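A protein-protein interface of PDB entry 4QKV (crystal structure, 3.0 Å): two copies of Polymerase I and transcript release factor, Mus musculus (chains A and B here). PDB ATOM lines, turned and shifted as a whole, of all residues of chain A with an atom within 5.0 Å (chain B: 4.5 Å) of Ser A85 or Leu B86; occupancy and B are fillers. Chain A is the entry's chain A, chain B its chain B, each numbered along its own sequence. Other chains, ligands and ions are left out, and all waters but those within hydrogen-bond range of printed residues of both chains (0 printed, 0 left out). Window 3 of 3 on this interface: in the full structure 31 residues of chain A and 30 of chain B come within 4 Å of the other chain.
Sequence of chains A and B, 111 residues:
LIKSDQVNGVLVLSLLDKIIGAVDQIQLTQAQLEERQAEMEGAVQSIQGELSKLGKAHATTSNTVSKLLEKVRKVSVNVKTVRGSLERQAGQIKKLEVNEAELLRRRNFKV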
ATOM      1  N   THR A  81     -25.625  19.570  21.362  1.00  0.00           N
ATOM      2  CA  THR A  81     -25.819  18.687  20.218  1.00  0.00           C
ATOM      3  C   THR A  81     -26.124  17.289  20.741  1.00  0.00           C
ATOM      4  O   THR A  81     -26.910  16.551  20.146  1.00  0.00           O
ATOM      5  CB  THR A  81     -24.594  18.624  19.291  1.00  0.00           C
ATOM      6  OG1 THR A  81     -23.558  17.855  19.914  1.00  0.00           O
ATOM      7  CG2 THR A  81     -24.084  20.020  18.959  1.00  0.00           C
ATOM      8  N   VAL A  82     -25.490  16.932  21.855  1.00  0.00           N
ATOM      9  CA  VAL A  82     -25.733  15.650  22.512  1.00  0.00           C
ATOM     10  C   VAL A  82     -27.130  15.636  23.129  1.00  0.00           C
ATOM     11  O   VAL A  82     -27.831  14.622  23.081  1.00  0.00           O
ATOM     12  CB  VAL A  82     -24.654  15.346  23.589  1.00  0.00           C
ATOM     13  CG1 VAL A  82     -25.215  14.493  24.710  1.00  0.00           C
ATOM     14  CG2 VAL A  82     -23.448  14.661  22.955  1.00  0.00           C
ATOM     15  N   ARG A  83     -27.545  16.764  23.693  1.00  0.00           N
ATOM     16  CA  ARG A  83     -28.929  16.884  24.121  1.00  0.00           C
ATOM     17  C   ARG A  83     -29.813  16.892  22.890  1.00  0.00           C
ATOM     18  O   ARG A  83     -30.886  16.314  22.899  1.00  0.00           O
ATOM     19  CB  ARG A  83     -29.159  18.138  24.962  1.00  0.00           C
ATOM     20  CG  ARG A  83     -29.418  17.826  26.423  1.00  0.00           C
ATOM     21  CD  ARG A  83     -30.510  18.690  27.012  1.00  0.00           C
ATOM     22  NE  ARG A  83     -31.787  18.479  26.345  1.00  0.00           N
ATOM     23  CZ  ARG A  83     -32.522  19.461  25.841  1.00  0.00           C
ATOM     24  NH1 ARG A  83     -32.097  20.716  25.936  1.00  0.00           N
ATOM     25  NH2 ARG A  83     -33.677  19.192  25.243  1.00  0.00           N
ATOM     26  N   GLY A  84     -29.337  17.528  21.824  1.00  0.00           N
ATOM     27  CA  GLY A  84     -30.075  17.601  20.574  1.00  0.00           C
ATOM     28  C   GLY A  84     -30.419  16.243  19.990  1.00  0.00           C
ATOM     29  O   GLY A  84     -31.548  16.011  19.555  1.00  0.00           O
ATOM     30  N   SER A  85     -29.445  15.338  19.986  1.00  0.00           N
ATOM     31  CA  SER A  85     -29.672  14.002  19.457  1.00  0.00           C
ATOM     32  C   SER A  85     -30.396  13.117  20.470  1.00  0.00           C
ATOM     33  O   SER A  85     -30.949  12.086  20.110  1.00  0.00           O
ATOM     34  CB  SER A  85     -28.351  13.355  19.036  1.00  0.00           C
ATOM     35  OG  SER A  85     -27.715  12.729  20.128  1.00  0.00           O
ATOM     36  N   LEU A  86     -30.412  13.527  21.732  1.00  0.00           N
ATOM     37  CA  LEU A  86     -31.050  12.739  22.785  1.00  0.00           C
ATOM     38  C   LEU A  86     -32.565  12.585  22.596  1.00  0.00           C
ATOM     39  O   LEU A  86     -33.084  11.474  22.659  1.00  0.00           O
ATOM     40  CB  LEU A  86     -30.767  13.363  24.151  1.00  0.00           C
ATOM     41  CG  LEU A  86     -31.408  12.681  25.354  1.00  0.00           C
ATOM     42  CD1 LEU A  86     -30.873  11.270  25.536  1.00  0.00           C
ATOM     43  CD2 LEU A  86     -31.165  13.538  26.580  1.00  0.00           C
ATOM     44  N   GLU A  87     -33.278  13.685  22.369  1.00  0.00           N
ATOM     45  CA  GLU A  87     -34.728  13.591  22.215  1.00  0.00           C
ATOM     46  C   GLU A  87     -35.117  13.243  20.790  1.00  0.00           C
ATOM     47  O   GLU A  87     -36.227  12.748  20.543  1.00  0.00           O
ATOM     48  CB  GLU A  87     -35.429  14.877  22.639  1.00  0.00           C
ATOM     49  CG  GLU A  87     -34.656  16.125  22.367  1.00  0.00           C
ATOM     50  CD  GLU A  87     -33.687  16.454  23.493  1.00  0.00           C
ATOM     51  OE1 GLU A  87     -33.458  15.576  24.361  1.00  0.00           O
ATOM     52  OE2 GLU A  87     -33.158  17.592  23.509  1.00  0.00           O
ATOM     53  N   ARG A  88     -34.217  13.503  19.847  1.00  0.00           N
ATOM     54  CA  ARG A  88     -34.414  12.937  18.527  1.00  0.00           C
ATOM     55  C   ARG A  88     -34.427  11.430  18.710  1.00  0.00           C
ATOM     56  O   ARG A  88     -35.245  10.751  18.118  1.00  0.00           O
ATOM     57  CB  ARG A  88     -33.344  13.384  17.528  1.00  0.00           C
ATOM     58  CG  ARG A  88     -33.754  14.616  16.723  1.00  0.00           C
ATOM     59  CD  ARG A  88     -32.636  15.640  16.638  1.00  0.00           C
ATOM     60  NE  ARG A  88     -33.142  17.008  16.521  1.00  0.00           N
ATOM     61  CZ  ARG A  88     -32.457  18.034  16.014  1.00  0.00           C
ATOM     62  NH1 ARG A  88     -31.223  17.860  15.558  1.00  0.00           N
ATOM     63  NH2 ARG A  88     -33.007  19.241  15.962  1.00  0.00           N
ATOM     64  N   GLN A  89     -33.557  10.909  19.569  1.00  0.00           N
ATOM     65  CA  GLN A  89     -33.607   9.484  19.898  1.00  0.00           C
ATOM     66  C   GLN A  89     -34.875   9.135  20.687  1.00  0.00           C
ATOM     67  O   GLN A  89     -35.459   8.061  20.496  1.00  0.00           O
ATOM     68  CB  GLN A  89     -32.361   9.060  20.686  1.00  0.00           C
ATOM     69  CG  GLN A  89     -31.077   9.028  19.864  1.00  0.00           C
ATOM     70  CD  GLN A  89     -30.131   7.921  20.293  1.00  0.00           C
ATOM     71  OE1 GLN A  89     -30.413   7.172  21.230  1.00  0.00           O
ATOM     72  NE2 GLN A  89     -29.002   7.811  19.604  1.00  0.00           N
ATOM     73  N   VAL B  82     -20.892   9.868  27.282  1.00  0.00           N
ATOM     74  CA  VAL B  82     -22.311  10.019  27.033  1.00  0.00           C
ATOM     75  C   VAL B  82     -22.579   9.973  25.524  1.00  0.00           C
ATOM     76  O   VAL B  82     -23.560   9.387  25.094  1.00  0.00           O
ATOM     77  CB  VAL B  82     -22.861  11.336  27.694  1.00  0.00           C
ATOM     78  CG1 VAL B  82     -22.573  12.570  26.865  1.00  0.00           C
ATOM     79  CG2 VAL B  82     -24.339  11.230  27.957  1.00  0.00           C
ATOM     80  N   ARG B  83     -21.690  10.545  24.718  1.00  0.00           N
ATOM     81  CA  ARG B  83     -21.878  10.506  23.277  1.00  0.00           C
ATOM     82  C   ARG B  83     -21.622   9.092  22.754  1.00  0.00           C
ATOM     83  O   ARG B  83     -22.403   8.555  21.964  1.00  0.00           O
ATOM     84  CB  ARG B  83     -20.955  11.498  22.574  1.00  0.00           C
ATOM     85  CG  ARG B  83     -21.006  11.353  21.062  1.00  0.00           C
ATOM     86  CD  ARG B  83     -19.878  12.082  20.356  1.00  0.00           C
ATOM     87  NE  ARG B  83     -19.796  13.487  20.739  1.00  0.00           N
ATOM     88  CZ  ARG B  83     -20.661  14.418  20.345  1.00  0.00           C
ATOM     89  NH1 ARG B  83     -21.694  14.084  19.569  1.00  0.00           N
ATOM     90  NH2 ARG B  83     -20.501  15.679  20.741  1.00  0.00           N
ATOM     91  N   GLY B  84     -20.509   8.510  23.193  1.00  0.00           N
ATOM     92  CA  GLY B  84     -20.151   7.161  22.821  1.00  0.00           C
ATOM     93  C   GLY B  84     -21.284   6.271  23.273  1.00  0.00           C
ATOM     94  O   GLY B  84     -21.719   5.374  22.554  1.00  0.00           O
ATOM     95  N   SER B  85     -21.796   6.533  24.466  1.00  0.00           N
ATOM     96  CA  SER B  85     -22.936   5.761  24.937  1.00  0.00           C
ATOM     97  C   SER B  85     -24.142   5.989  24.038  1.00  0.00           C
ATOM     98  O   SER B  85     -24.958   5.099  23.836  1.00  0.00           O
ATOM     99  CB  SER B  85     -23.281   6.131  26.377  1.00  0.00           C
ATOM    100  OG  SER B  85     -24.126   5.157  26.953  1.00  0.00           O
ATOM    101  N   LEU B  86     -24.224   7.190  23.478  1.00  0.00           N
ATOM    102  CA  LEU B  86     -25.413   7.625  22.763  1.00  0.00           C
ATOM    103  C   LEU B  86     -25.582   6.906  21.432  1.00  0.00           C
ATOM    104  O   LEU B  86     -26.612   6.279  21.201  1.00  0.00           O
ATOM    105  CB  LEU B  86     -25.367   9.137  22.554  1.00  0.00           C
ATOM    106  CG  LEU B  86     -26.695   9.881  22.522  1.00  0.00           C
ATOM    107  CD1 LEU B  86     -26.499  11.300  23.014  1.00  0.00           C
ATOM    108  CD2 LEU B  86     -27.195   9.904  21.116  1.00  0.00           C
ATOM    109  N   GLU B  87     -24.594   6.984  20.548  1.00  0.00           N
ATOM    110  CA  GLU B  87     -24.772   6.336  19.252  1.00  0.00           C
ATOM    111  C   GLU B  87     -24.406   4.850  19.306  1.00  0.00           C
ATOM    112  O   GLU B  87     -24.389   4.177  18.281  1.00  0.00           O
ATOM    113  CB  GLU B  87     -23.995   7.063  18.137  1.00  0.00           C
ATOM    114  CG  GLU B  87     -22.577   6.586  17.839  1.00  0.00           C
ATOM    115  CD  GLU B  87     -21.542   7.219  18.752  1.00  0.00           C
ATOM    116  OE1 GLU B  87     -21.685   7.111  19.982  1.00  0.00           O
ATOM    117  OE2 GLU B  87     -20.597   7.855  18.243  1.00  0.00           O
ATOM    118  N   ARG B  88     -24.141   4.328  20.503  1.00  0.00           N
ATOM    119  CA  ARG B  88     -24.224   2.881  20.702  1.00  0.00           C
ATOM    120  C   ARG B  88     -25.695   2.528  20.772  1.00  0.00           C
ATOM    121  O   ARG B  88     -26.122   1.471  20.315  1.00  0.00           O
ATOM    122  CB  ARG B  88     -23.513   2.420  21.971  1.00  0.00           C
ATOM    123  CG  ARG B  88     -22.017   2.466  21.874  1.00  0.00           C
ATOM    124  CD  ARG B  88     -21.350   2.025  23.170  1.00  0.00           C
ATOM    125  NE  ARG B  88     -20.115   2.766  23.435  1.00  0.00           N
ATOM    126  CZ  ARG B  88     -19.021   2.734  22.672  1.00  0.00           C
ATOM    127  NH1 ARG B  88     -18.978   1.991  21.572  1.00  0.00           N
ATOM    128  NH2 ARG B  88     -17.956   3.454  23.014  1.00  0.00           N
ATOM    129  N   GLN B  89     -26.469   3.437  21.356  1.00  0.00           N
ATOM    130  CA  GLN B  89     -27.911   3.275  21.410  1.00  0.00           C
ATOM    131  C   GLN B  89     -28.509   3.518  20.033  1.00  0.00           C
ATOM    132  O   GLN B  89     -29.392   2.787  19.621  1.00  0.00           O
ATOM    133  CB  GLN B  89     -28.537   4.222  22.440  1.00  0.00           C
ATOM    134  CG  GLN B  89     -28.076   3.976  23.877  1.00  0.00           C
ATOM    135  CD  GLN B  89     -29.089   4.429  24.919  1.00  0.00           C
ATOM    136  OE1 GLN B  89     -30.076   5.098  24.602  1.00  0.00           O
ATOM    137  NE2 GLN B  89     -28.854   4.052  26.166  1.00  0.00           N
ATOM    138  N   ALA B  90     -28.031   4.540  19.326  1.00  0.00           N
ATOM    139  CA  ALA B  90     -28.503   4.810  17.971  1.00  0.00           C
ATOM    140  C   ALA B  90     -28.367   3.555  17.113  1.00  0.00           C
ATOM    141  O   ALA B  90     -29.256   3.225  16.323  1.00  0.00           O
ATOM    142  CB  ALA B  90     -27.735   5.961  17.355  1.00  0.00           C
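NH2 of Arg B83 touches OG1 of Thr A81, 3.8 Å away.
Val B82 touches Val A82.
Arg B83 touches Val A82 (NH2 to CG2, 3.8 Å).
Val A82 touches Leu B86 (O to CD1, 3.6 Å).
Leu B86 touches Ser A85.
Gln B89 touches Gln A89.
Val A82 touches its own counterpart, Val B82.
Val A82 touches Leu B86, but with the chains exchanged Leu A86 does not touch Val B82 (7.0 Å).
Ser A85 touches Leu B86, but with the chains exchanged Leu A86 does not touch Ser B85 (8.7 Å).
Gln A89 touches its own counterpart, Gln B89.
Positions printed for both chains: 82, 83, 84, 85, 86, 87, 88 and 89.
Hydrophobic or aromatic side chains of chain A that line the printed part of chain B: Val A82.
Of the 9 printed residues of chain B, 5 touch a printed residue of chain A.
Among the printed residues, 8 pairs touch across the chains.
The backbone carbonyl oxygen (O) of Leu B86 sits close to the side-chain amide nitrogen (NE2) of Gln A89 (3.3 Å).
N of Ala B90 lies close to NE2 of Gln A89 (3.4 Å).
OE1 of Glu B87 lies close to O of Arg B83.
Of chain B, only Leu B86 (3.0 Å) comes within 4 Å of Ser A85.
Leu A86 touches none of the printed residues of chain B.
Printed residues of chain B within 4 Å of Gln A89: Leu B86, Gln B89 and Ala B90.
Leu B86 touches just these residues of chain A: Val A82, Ser A85 and Gln A89.
Printed residues of chain A within 4 Å of Ala B90: Gln A89.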
